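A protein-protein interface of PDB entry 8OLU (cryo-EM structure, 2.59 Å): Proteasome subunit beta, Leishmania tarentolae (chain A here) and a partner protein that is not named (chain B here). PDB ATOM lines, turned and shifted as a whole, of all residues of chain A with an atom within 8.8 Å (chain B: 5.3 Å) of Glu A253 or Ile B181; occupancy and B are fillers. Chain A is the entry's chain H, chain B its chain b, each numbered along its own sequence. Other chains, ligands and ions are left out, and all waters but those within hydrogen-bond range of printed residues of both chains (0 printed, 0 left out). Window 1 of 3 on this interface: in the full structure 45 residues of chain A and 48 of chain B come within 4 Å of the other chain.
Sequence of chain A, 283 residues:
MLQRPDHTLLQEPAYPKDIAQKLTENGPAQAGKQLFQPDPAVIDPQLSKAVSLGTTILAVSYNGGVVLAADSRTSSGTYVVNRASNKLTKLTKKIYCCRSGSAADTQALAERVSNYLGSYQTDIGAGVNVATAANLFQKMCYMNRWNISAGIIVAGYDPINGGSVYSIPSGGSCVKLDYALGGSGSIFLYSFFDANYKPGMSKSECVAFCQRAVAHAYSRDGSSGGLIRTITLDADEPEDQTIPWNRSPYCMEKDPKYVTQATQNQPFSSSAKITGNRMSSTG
The backbone carbonyl oxygen of Ala B30 lies within hydrogen-bond range of the guanidinium group of Arg A220 (2.6 Å). N of Asn B182 is in hydrogen-bond range of OE2 of Glu A253.
OG1 of Thr B22 sits at hydrogen-bond distance from O of Pro B33, at 2.6 Å. The backbone NH (N) of Thr B22 is in hydrogen-bond range of the backbone carbonyl oxygen (O) of Lys B183, at 3.1 Å. The backbone carbonyl oxygen (O) of Pro B33 lies within hydrogen-bond range of the side-chain amino group (NZ) of Lys B183, 2.9 Å away. The side-chain hydroxyl of Ser A219 sits at hydrogen-bond distance from the backbone carbonyl oxygen of Ala A215 (2.7 Å). The guanidinium group (NH2) of Arg A220 lies close to the side-chain sulfur (SD) of Met A252, at 3.4 Å. The guanidinium group of Arg A220 lies within hydrogen-bond range of the side-chain hydroxyl of Tyr A258 (3.2 Å).
Ala B30 touches Ser A219 (CB to O, 3.8 Å). CE2 of Trp A245 touches CZ of Phe B174 (3.7 Å). ND2 of Asn B182 touches CZ3 of Trp A245 (3.7 Å). Met A252 touches Ala B30. Pro B33 touches Met A252 (CB to CE, 3.6 Å). OE2 of Glu A253 touches CE1 of Phe B174, 3.9 Å away. CA of Ile B181 touches OE2 of Glu A253, 3.5 Å away. Pro B33 touches Tyr A258. Lys B183 touches Tyr A258 (NZ to O, 3.5 Å). Thr B22 touches Gln A261.
Printed residues of chain B within 4 Å of Glu A253: Phe B174 (3.9 Å), Ile B181 (3.5 Å) and Asn B182 (3.0 Å). Of chain A, only Glu A253 comes within 4 Å of Ile B181. No residue of chain A comes within 4 Å of Ala B180. Of the printed residues of chain A, Lys B183 touches Tyr A258 (3.5 Å). Of the printed residues of chain B, Gln A261 touches Thr B22. Of the printed residues of chain B, Arg A220 touches Ala B30. The nearest residue of chain A that does not touch Ile B181 is Met A252 (4.6 Å).
Of the 13 printed residues of chain B, 7 touch a printed residue of chain A. Among the printed residues, 12 pairs touch across the chains.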
ATOM      1  N   ARG A  73      22.774  -6.453 -29.072  1.00  0.00           N
ATOM      2  CA  ARG A  73      23.758  -6.252 -28.042  1.00  0.00           C
ATOM      3  C   ARG A  73      24.644  -7.463 -27.820  1.00  0.00           C
ATOM      4  O   ARG A  73      24.140  -8.548 -27.659  1.00  0.00           O
ATOM      5  CB  ARG A  73      23.010  -6.015 -26.748  1.00  0.00           C
ATOM      6  CG  ARG A  73      23.800  -6.296 -25.481  1.00  0.00           C
ATOM      7  CD  ARG A  73      23.033  -5.861 -24.224  1.00  0.00           C
ATOM      8  NE  ARG A  73      22.481  -4.531 -24.353  1.00  0.00           N
ATOM      9  CZ  ARG A  73      21.949  -3.872 -23.366  1.00  0.00           C
ATOM     10  NH1 ARG A  73      21.726  -4.436 -22.205  1.00  0.00           N
ATOM     11  NH2 ARG A  73      21.656  -2.621 -23.575  1.00  0.00           N
ATOM     12  N   ALA A 215      11.394  -6.065 -29.142  1.00  0.00           N
ATOM     13  CA  ALA A 215      11.413  -4.989 -28.171  1.00  0.00           C
ATOM     14  C   ALA A 215      10.960  -5.421 -26.781  1.00  0.00           C
ATOM     15  O   ALA A 215      11.488  -5.017 -25.772  1.00  0.00           O
ATOM     16  CB  ALA A 215      10.552  -3.895 -28.634  1.00  0.00           C
ATOM     17  N   TYR A 218      13.803  -7.443 -25.292  1.00  0.00           N
ATOM     18  CA  TYR A 218      14.978  -6.776 -24.794  1.00  0.00           C
ATOM     19  C   TYR A 218      14.649  -5.703 -23.765  1.00  0.00           C
ATOM     20  O   TYR A 218      15.550  -5.255 -23.085  1.00  0.00           O
ATOM     21  CB  TYR A 218      15.787  -6.269 -25.983  1.00  0.00           C
ATOM     22  CG  TYR A 218      15.391  -5.002 -26.675  1.00  0.00           C
ATOM     23  CD1 TYR A 218      14.691  -3.979 -26.117  1.00  0.00           C
ATOM     24  CD2 TYR A 218      15.806  -4.844 -27.964  1.00  0.00           C
ATOM     25  CE1 TYR A 218      14.350  -2.846 -26.851  1.00  0.00           C
ATOM     26  CE2 TYR A 218      15.506  -3.707 -28.687  1.00  0.00           C
ATOM     27  CZ  TYR A 218      14.769  -2.686 -28.142  1.00  0.00           C
ATOM     28  OH  TYR A 218      14.602  -1.591 -28.999  1.00  0.00           O
ATOM     29  N   SER A 219      13.381  -5.422 -23.540  1.00  0.00           N
ATOM     30  CA  SER A 219      13.005  -4.552 -22.449  1.00  0.00           C
ATOM     31  C   SER A 219      13.101  -5.246 -21.102  1.00  0.00           C
ATOM     32  O   SER A 219      13.331  -4.598 -20.118  1.00  0.00           O
ATOM     33  CB  SER A 219      11.688  -3.976 -22.709  1.00  0.00           C
ATOM     34  OG  SER A 219      11.830  -3.116 -23.872  1.00  0.00           O
ATOM     35  N   ARG A 220      13.144  -6.563 -21.096  1.00  0.00           N
ATOM     36  CA  ARG A 220      13.272  -7.292 -19.880  1.00  0.00           C
ATOM     37  C   ARG A 220      14.575  -8.052 -19.785  1.00  0.00           C
ATOM     38  O   ARG A 220      15.003  -8.305 -18.690  1.00  0.00           O
ATOM     39  CB  ARG A 220      12.096  -8.262 -19.823  1.00  0.00           C
ATOM     40  CG  ARG A 220      10.732  -7.596 -19.606  1.00  0.00           C
ATOM     41  CD  ARG A 220      10.640  -7.066 -18.224  1.00  0.00           C
ATOM     42  NE  ARG A 220       9.316  -6.673 -17.812  1.00  0.00           N
ATOM     43  CZ  ARG A 220       9.076  -6.131 -16.624  1.00  0.00           C
ATOM     44  NH1 ARG A 220       9.942  -6.146 -15.633  1.00  0.00           N
ATOM     45  NH2 ARG A 220       7.956  -5.478 -16.485  1.00  0.00           N
ATOM     46  N   ASP A 221      15.155  -8.523 -20.881  1.00  0.00           N
ATOM     47  CA  ASP A 221      16.431  -9.208 -20.799  1.00  0.00           C
ATOM     48  C   ASP A 221      17.516  -8.144 -20.752  1.00  0.00           C
ATOM     49  O   ASP A 221      17.586  -7.252 -21.600  1.00  0.00           O
ATOM     50  CB  ASP A 221      16.654 -10.158 -21.956  1.00  0.00           C
ATOM     51  CG  ASP A 221      17.925 -11.023 -21.852  1.00  0.00           C
ATOM     52  OD1 ASP A 221      18.416 -11.268 -20.672  1.00  0.00           O
ATOM     53  OD2 ASP A 221      18.494 -11.455 -22.953  1.00  0.00           O
ATOM     54  N   GLY A 222      18.299  -8.184 -19.677  1.00  0.00           N
ATOM     55  CA  GLY A 222      19.465  -7.335 -19.503  1.00  0.00           C
ATOM     56  C   GLY A 222      20.528  -7.643 -20.544  1.00  0.00           C
ATOM     57  O   GLY A 222      21.321  -6.784 -20.910  1.00  0.00           O
ATOM     58  N   TRP A 245      17.043   2.324 -30.939  1.00  0.00           N
ATOM     59  CA  TRP A 245      16.388   2.018 -29.688  1.00  0.00           C
ATOM     60  C   TRP A 245      15.350   3.051 -29.344  1.00  0.00           C
ATOM     61  O   TRP A 245      14.416   2.774 -28.608  1.00  0.00           O
ATOM     62  CB  TRP A 245      17.372   1.898 -28.524  1.00  0.00           C
ATOM     63  CG  TRP A 245      16.683   1.628 -27.225  1.00  0.00           C
ATOM     64  CD1 TRP A 245      16.246   0.434 -26.760  1.00  0.00           C
ATOM     65  CD2 TRP A 245      16.250   2.610 -26.295  1.00  0.00           C
ATOM     66  NE1 TRP A 245      15.602   0.614 -25.564  1.00  0.00           N
ATOM     67  CE2 TRP A 245      15.585   1.943 -25.267  1.00  0.00           C
ATOM     68  CE3 TRP A 245      16.306   3.992 -26.278  1.00  0.00           C
ATOM     69  CZ2 TRP A 245      14.949   2.611 -24.238  1.00  0.00           C
ATOM     70  CZ3 TRP A 245      15.690   4.674 -25.247  1.00  0.00           C
ATOM     71  CH2 TRP A 245      15.032   3.987 -24.235  1.00  0.00           C
ATOM     72  N   SER A 248      12.064   2.352 -30.709  1.00  0.00           N
ATOM     73  CA  SER A 248      11.599   1.040 -30.396  1.00  0.00           C
ATOM     74  C   SER A 248      10.092   1.099 -30.208  1.00  0.00           C
ATOM     75  O   SER A 248       9.563   1.971 -29.525  1.00  0.00           O
ATOM     76  CB  SER A 248      12.278   0.531 -29.193  1.00  0.00           C
ATOM     77  OG  SER A 248      11.809  -0.762 -28.788  1.00  0.00           O
ATOM     78  N   TYR A 250       8.413  -0.804 -28.362  1.00  0.00           N
ATOM     79  CA  TYR A 250       8.050  -0.901 -26.963  1.00  0.00           C
ATOM     80  C   TYR A 250       9.265  -0.659 -26.105  1.00  0.00           C
ATOM     81  O   TYR A 250      10.330  -1.170 -26.381  1.00  0.00           O
ATOM     82  CB  TYR A 250       7.461  -2.273 -26.596  1.00  0.00           C
ATOM     83  CG  TYR A 250       7.094  -2.387 -25.133  1.00  0.00           C
ATOM     84  CD1 TYR A 250       6.005  -1.727 -24.614  1.00  0.00           C
ATOM     85  CD2 TYR A 250       7.938  -3.011 -24.228  1.00  0.00           C
ATOM     86  CE1 TYR A 250       5.674  -1.782 -23.272  1.00  0.00           C
ATOM     87  CE2 TYR A 250       7.670  -2.987 -22.866  1.00  0.00           C
ATOM     88  CZ  TYR A 250       6.521  -2.388 -22.381  1.00  0.00           C
ATOM     89  OH  TYR A 250       6.255  -2.465 -21.051  1.00  0.00           O
ATOM     90  N   CYS A 251       9.085   0.090 -25.021  1.00  0.00           N
ATOM     91  CA  CYS A 251       9.983  -0.081 -23.885  1.00  0.00           C
ATOM     92  C   CYS A 251       9.306   0.318 -22.589  1.00  0.00           C
ATOM     93  O   CYS A 251       8.418   1.163 -22.608  1.00  0.00           O
ATOM     94  CB  CYS A 251      11.227   0.774 -24.077  1.00  0.00           C
ATOM     95  SG  CYS A 251      10.850   2.531 -24.189  1.00  0.00           S
ATOM     96  N   MET A 252       9.799  -0.244 -21.489  1.00  0.00           N
ATOM     97  CA  MET A 252       9.294   0.040 -20.155  1.00  0.00           C
ATOM     98  C   MET A 252       9.455   1.500 -19.789  1.00  0.00           C
ATOM     99  O   MET A 252       8.619   2.057 -19.099  1.00  0.00           O
ATOM    100  CB  MET A 252      10.032  -0.822 -19.127  1.00  0.00           C
ATOM    101  CG  MET A 252       9.569  -2.256 -19.295  1.00  0.00           C
ATOM    102  SD  MET A 252      10.094  -3.379 -17.994  1.00  0.00           S
ATOM    103  CE  MET A 252      11.766  -2.811 -17.618  1.00  0.00           C
ATOM    104  N   GLU A 253      10.487   2.143 -20.276  1.00  0.00           N
ATOM    105  CA  GLU A 253      10.734   3.528 -19.942  1.00  0.00           C
ATOM    106  C   GLU A 253       9.705   4.448 -20.610  1.00  0.00           C
ATOM    107  O   GLU A 253       9.825   5.662 -20.522  1.00  0.00           O
ATOM    108  CB  GLU A 253      12.139   3.923 -20.438  1.00  0.00           C
ATOM    109  CG  GLU A 253      13.324   2.993 -20.052  1.00  0.00           C
ATOM    110  CD  GLU A 253      13.838   1.819 -20.921  1.00  0.00           C
ATOM    111  OE1 GLU A 253      13.002   0.880 -21.239  1.00  0.00           O
ATOM    112  OE2 GLU A 253      15.116   1.723 -21.159  1.00  0.00           O
ATOM    113  N   LYS A 254       8.771   3.924 -21.381  1.00  0.00           N
ATOM    114  CA  LYS A 254       7.805   4.776 -22.036  1.00  0.00           C
ATOM    115  C   LYS A 254       6.404   4.195 -21.977  1.00  0.00           C
ATOM    116  O   LYS A 254       5.472   4.806 -22.482  1.00  0.00           O
ATOM    117  CB  LYS A 254       8.191   4.980 -23.504  1.00  0.00           C
ATOM    118  CG  LYS A 254       9.387   5.906 -23.715  1.00  0.00           C
ATOM    119  CD  LYS A 254      10.015   5.875 -25.086  1.00  0.00           C
ATOM    120  CE  LYS A 254      11.313   6.668 -25.103  1.00  0.00           C
ATOM    121  NZ  LYS A 254      11.978   6.680 -26.439  1.00  0.00           N
ATOM    122  N   ASP A 255       6.273   2.995 -21.420  1.00  0.00           N
ATOM    123  CA  ASP A 255       4.992   2.388 -21.139  1.00  0.00           C
ATOM    124  C   ASP A 255       4.332   3.218 -20.047  1.00  0.00           C
ATOM    125  O   ASP A 255       4.934   3.417 -18.996  1.00  0.00           O
ATOM    126  CB  ASP A 255       5.191   0.934 -20.702  1.00  0.00           C
ATOM    127  CG  ASP A 255       3.917   0.087 -20.618  1.00  0.00           C
ATOM    128  OD1 ASP A 255       2.798   0.697 -20.627  1.00  0.00           O
ATOM    129  OD2 ASP A 255       4.027  -1.198 -20.566  1.00  0.00           O
ATOM    130  N   PRO A 256       3.101   3.724 -20.217  1.00  0.00           N
ATOM    131  CA  PRO A 256       2.482   4.531 -19.162  1.00  0.00           C
ATOM    132  C   PRO A 256       2.180   3.792 -17.871  1.00  0.00           C
ATOM    133  O   PRO A 256       2.153   4.392 -16.797  1.00  0.00           O
ATOM    134  CB  PRO A 256       1.186   5.020 -19.784  1.00  0.00           C
ATOM    135  CG  PRO A 256       1.406   4.801 -21.314  1.00  0.00           C
ATOM    136  CD  PRO A 256       2.270   3.572 -21.422  1.00  0.00           C
ATOM    137  N   LYS A 257       2.112   2.474 -17.919  1.00  0.00           N
ATOM    138  CA  LYS A 257       1.871   1.784 -16.671  1.00  0.00           C
ATOM    139  C   LYS A 257       3.105   1.605 -15.808  1.00  0.00           C
ATOM    140  O   LYS A 257       3.007   0.926 -14.804  1.00  0.00           O
ATOM    141  CB  LYS A 257       1.262   0.414 -16.923  1.00  0.00           C
ATOM    142  CG  LYS A 257       2.208  -0.635 -17.460  1.00  0.00           C
ATOM    143  CD  LYS A 257       1.595  -2.020 -17.517  1.00  0.00           C
ATOM    144  CE  LYS A 257       2.343  -2.928 -18.478  1.00  0.00           C
ATOM    145  NZ  LYS A 257       1.888  -2.714 -19.869  1.00  0.00           N
ATOM    146  N   TYR A 258       4.260   2.144 -16.199  1.00  0.00           N
ATOM    147  CA  TYR A 258       5.460   2.072 -15.377  1.00  0.00           C
ATOM    148  C   TYR A 258       5.982   3.464 -15.101  1.00  0.00           C
ATOM    149  O   TYR A 258       7.145   3.609 -14.741  1.00  0.00           O
ATOM    150  CB  TYR A 258       6.573   1.240 -16.049  1.00  0.00           C
ATOM    151  CG  TYR A 258       6.234  -0.214 -16.230  1.00  0.00           C
ATOM    152  CD1 TYR A 258       5.857  -0.989 -15.146  1.00  0.00           C
ATOM    153  CD2 TYR A 258       6.236  -0.797 -17.481  1.00  0.00           C
ATOM    154  CE1 TYR A 258       5.462  -2.312 -15.310  1.00  0.00           C
ATOM    155  CE2 TYR A 258       5.817  -2.114 -17.673  1.00  0.00           C
ATOM    156  CZ  TYR A 258       5.427  -2.889 -16.582  1.00  0.00           C
ATOM    157  OH  TYR A 258       5.015  -4.201 -16.739  1.00  0.00           O
ATOM    158  N   VAL A 259       5.136   4.473 -15.290  1.00  0.00           N
ATOM    159  CA  VAL A 259       5.486   5.849 -14.995  1.00  0.00           C
ATOM    160  C   VAL A 259       5.328   6.162 -13.514  1.00  0.00           C
ATOM    161  O   VAL A 259       6.094   6.962 -12.968  1.00  0.00           O
ATOM    162  CB  VAL A 259       4.601   6.819 -15.782  1.00  0.00           C
ATOM    163  CG1 VAL A 259       4.810   8.242 -15.323  1.00  0.00           C
ATOM    164  CG2 VAL A 259       4.860   6.714 -17.265  1.00  0.00           C
ATOM    165  N   GLN A 261       5.978   5.840  -9.772  1.00  0.00           N
ATOM    166  CA  GLN A 261       7.007   5.136  -9.042  1.00  0.00           C
ATOM    167  C   GLN A 261       6.379   4.312  -7.938  1.00  0.00           C
ATOM    168  O   GLN A 261       5.442   4.732  -7.272  1.00  0.00           O
ATOM    169  CB  GLN A 261       8.063   6.096  -8.518  1.00  0.00           C
ATOM    170  CG  GLN A 261       8.977   6.607  -9.618  1.00  0.00           C
ATOM    171  CD  GLN A 261      10.328   7.034  -9.116  1.00  0.00           C
ATOM    172  OE1 GLN A 261      10.472   8.084  -8.499  1.00  0.00           O
ATOM    173  NE2 GLN A 261      11.336   6.226  -9.384  1.00  0.00           N
ATOM    174  N   ASP B  21      19.507   5.146 -12.078  1.00  0.00           N
ATOM    175  CA  ASP B  21      18.371   4.633 -12.840  1.00  0.00           C
ATOM    176  C   ASP B  21      17.329   4.156 -11.865  1.00  0.00           C
ATOM    177  O   ASP B  21      17.632   3.893 -10.737  1.00  0.00           O
ATOM    178  CB  ASP B  21      18.739   3.542 -13.854  1.00  0.00           C
ATOM    179  CG  ASP B  21      19.227   2.234 -13.223  1.00  0.00           C
ATOM    180  OD1 ASP B  21      18.976   2.051 -11.960  1.00  0.00           O
ATOM    181  OD2 ASP B  21      19.909   1.381 -13.972  1.00  0.00           O
ATOM    182  N   THR B  22      16.101   4.074 -12.299  1.00  0.00           N
ATOM    183  CA  THR B  22      15.048   3.668 -11.434  1.00  0.00           C
ATOM    184  C   THR B  22      14.767   2.218 -11.626  1.00  0.00           C
ATOM    185  O   THR B  22      13.642   1.850 -11.771  1.00  0.00           O
ATOM    186  CB  THR B  22      13.820   4.496 -11.751  1.00  0.00           C
ATOM    187  OG1 THR B  22      13.244   4.100 -12.992  1.00  0.00           O
ATOM    188  CG2 THR B  22      14.197   5.963 -11.691  1.00  0.00           C
ATOM    189  N   LEU B  23      15.757   1.390 -11.543  1.00  0.00           N
ATOM    190  CA  LEU B  23      15.516   0.056 -11.964  1.00  0.00           C
ATOM    191  C   LEU B  23      16.075  -0.918 -10.982  1.00  0.00           C
ATOM    192  O   LEU B  23      17.206  -0.791 -10.624  1.00  0.00           O
ATOM    193  CB  LEU B  23      16.163  -0.214 -13.303  1.00  0.00           C
ATOM    194  CG  LEU B  23      16.247  -1.713 -13.614  1.00  0.00           C
ATOM    195  CD1 LEU B  23      14.978  -2.241 -14.232  1.00  0.00           C
ATOM    196  CD2 LEU B  23      17.362  -2.039 -14.583  1.00  0.00           C
ATOM    197  N   ALA B  30      15.209  -7.433 -16.010  1.00  0.00           N
ATOM    198  CA  ALA B  30      14.875  -6.102 -15.557  1.00  0.00           C
ATOM    199  C   ALA B  30      13.516  -6.136 -14.906  1.00  0.00           C
ATOM    200  O   ALA B  30      12.553  -6.248 -15.621  1.00  0.00           O
ATOM    201  CB  ALA B  30      14.860  -5.169 -16.716  1.00  0.00           C
ATOM    202  N   PRO B  33      11.048  -1.283 -13.205  1.00  0.00           N
ATOM    203  CA  PRO B  33      11.657  -0.096 -13.735  1.00  0.00           C
ATOM    204  C   PRO B  33      11.204   1.208 -13.160  1.00  0.00           C
ATOM    205  O   PRO B  33      11.504   2.251 -13.695  1.00  0.00           O
ATOM    206  CB  PRO B  33      11.142  -0.246 -15.134  1.00  0.00           C
ATOM    207  CG  PRO B  33       9.780  -0.721 -14.946  1.00  0.00           C
ATOM    208  CD  PRO B  33       9.966  -1.839 -13.979  1.00  0.00           C
ATOM    209  N   PHE B 174      23.797   4.141 -19.911  1.00  0.00           N
ATOM    210  CA  PHE B 174      22.692   3.518 -20.593  1.00  0.00           C
ATOM    211  C   PHE B 174      23.201   2.669 -21.738  1.00  0.00           C
ATOM    212  O   PHE B 174      22.709   1.607 -21.928  1.00  0.00           O
ATOM    213  CB  PHE B 174      21.705   4.530 -21.149  1.00  0.00           C
ATOM    214  CG  PHE B 174      20.615   3.805 -21.880  1.00  0.00           C
ATOM    215  CD1 PHE B 174      19.892   2.818 -21.252  1.00  0.00           C
ATOM    216  CD2 PHE B 174      20.309   4.118 -23.189  1.00  0.00           C
ATOM    217  CE1 PHE B 174      18.883   2.149 -21.925  1.00  0.00           C
ATOM    218  CE2 PHE B 174      19.236   3.503 -23.815  1.00  0.00           C
ATOM    219  CZ  PHE B 174      18.565   2.485 -23.199  1.00  0.00           C
ATOM    220  N   ARG B 179      22.443  -3.961 -17.436  1.00  0.00           N
ATOM    221  CA  ARG B 179      21.299  -3.928 -16.578  1.00  0.00           C
ATOM    222  C   ARG B 179      20.975  -2.472 -16.289  1.00  0.00           C
ATOM    223  O   ARG B 179      21.351  -1.947 -15.246  1.00  0.00           O
ATOM    224  CB  ARG B 179      21.686  -4.709 -15.320  1.00  0.00           C
ATOM    225  CG  ARG B 179      21.852  -6.200 -15.573  1.00  0.00           C
ATOM    226  CD  ARG B 179      22.382  -7.064 -14.426  1.00  0.00           C
ATOM    227  NE  ARG B 179      22.788  -8.309 -15.108  1.00  0.00           N
ATOM    228  CZ  ARG B 179      23.290  -9.404 -14.522  1.00  0.00           C
ATOM    229  NH1 ARG B 179      23.551 -10.486 -15.231  1.00  0.00           N
ATOM    230  NH2 ARG B 179      23.450  -9.424 -13.210  1.00  0.00           N
ATOM    231  N   ALA B 180      20.403  -1.790 -17.235  1.00  0.00           N
ATOM    232  CA  ALA B 180      20.086  -0.383 -17.075  1.00  0.00           C
ATOM    233  C   ALA B 180      18.851  -0.042 -17.892  1.00  0.00           C
ATOM    234  O   ALA B 180      18.385  -0.833 -18.736  1.00  0.00           O
ATOM    235  CB  ALA B 180      21.197   0.507 -17.521  1.00  0.00           C
ATOM    236  N   ILE B 181      18.298   1.106 -17.564  1.00  0.00           N
ATOM    237  CA  ILE B 181      17.217   1.598 -18.343  1.00  0.00           C
ATOM    238  C   ILE B 181      17.407   3.049 -18.512  1.00  0.00           C
ATOM    239  O   ILE B 181      18.055   3.675 -17.708  1.00  0.00           O
ATOM    240  CB  ILE B 181      15.864   1.327 -17.713  1.00  0.00           C
ATOM    241  CG1 ILE B 181      15.731   1.924 -16.319  1.00  0.00           C
ATOM    242  CG2 ILE B 181      15.543  -0.147 -17.683  1.00  0.00           C
ATOM    243  CD1 ILE B 181      14.272   1.762 -15.851  1.00  0.00           C
ATOM    244  N   ASN B 182      16.775   3.571 -19.511  1.00  0.00           N
ATOM    245  CA  ASN B 182      16.871   4.990 -19.733  1.00  0.00           C
ATOM    246  C   ASN B 182      15.757   5.655 -18.939  1.00  0.00           C
ATOM    247  O   ASN B 182      14.816   6.162 -19.530  1.00  0.00           O
ATOM    248  CB  ASN B 182      16.839   5.228 -21.240  1.00  0.00           C
ATOM    249  CG  ASN B 182      17.036   6.667 -21.553  1.00  0.00           C
ATOM    250  OD1 ASN B 182      17.194   7.472 -20.650  1.00  0.00           O
ATOM    251  ND2 ASN B 182      17.171   6.966 -22.815  1.00  0.00           N
ATOM    252  N   LYS B 183      15.828   5.559 -17.618  1.00  0.00           N
ATOM    253  CA  LYS B 183      14.967   6.329 -16.738  1.00  0.00           C
ATOM    254  C   LYS B 183      15.770   6.631 -15.506  1.00  0.00           C
ATOM    255  O   LYS B 183      16.209   5.674 -14.904  1.00  0.00           O
ATOM    256  CB  LYS B 183      13.692   5.594 -16.276  1.00  0.00           C
ATOM    257  CG  LYS B 183      12.574   6.556 -15.883  1.00  0.00           C
ATOM    258  CD  LYS B 183      11.195   6.303 -16.527  1.00  0.00           C
ATOM    259  CE  LYS B 183      10.288   5.404 -15.671  1.00  0.00           C
ATOM    260  NZ  LYS B 183      10.486   3.912 -15.856  1.00  0.00           N
ATOM    261  N   PHE B 184      15.939   7.896 -15.149  1.00  0.00           N
ATOM    262  CA  PHE B 184      16.860   8.280 -14.092  1.00  0.00           C
ATOM    263  C   PHE B 184      16.213   9.249 -13.140  1.00  0.00           C
ATOM    264  O   PHE B 184      15.346  10.002 -13.521  1.00  0.00           O
ATOM    265  CB  PHE B 184      18.020   9.077 -14.656  1.00  0.00           C
ATOM    266  CG  PHE B 184      18.775   8.236 -15.614  1.00  0.00           C
ATOM    267  CD1 PHE B 184      19.596   7.222 -15.141  1.00  0.00           C
ATOM    268  CD2 PHE B 184      18.519   8.309 -16.986  1.00  0.00           C
ATOM    269  CE1 PHE B 184      20.236   6.384 -16.033  1.00  0.00           C
ATOM    270  CE2 PHE B 184      19.120   7.410 -17.872  1.00  0.00           C
ATOM    271  CZ  PHE B 184      19.946   6.437 -17.383  1.00  0.00           C
ATOM    272  N   ASP B 201      14.547  10.907 -18.849  1.00  0.00           N
ATOM    273  CA  ASP B 201      15.298  10.082 -19.778  1.00  0.00           C
ATOM    274  C   ASP B 201      16.318  10.950 -20.488  1.00  0.00           C
ATOM    275  O   ASP B 201      16.295  12.159 -20.421  1.00  0.00           O
ATOM    276  CB  ASP B 201      14.371   9.367 -20.745  1.00  0.00           C
ATOM    277  CG  ASP B 201      13.395  10.319 -21.431  1.00  0.00           C
ATOM    278  OD1 ASP B 201      13.526  11.561 -21.178  1.00  0.00           O
ATOM    279  OD2 ASP B 201      12.496   9.836 -22.212  1.00  0.00           O
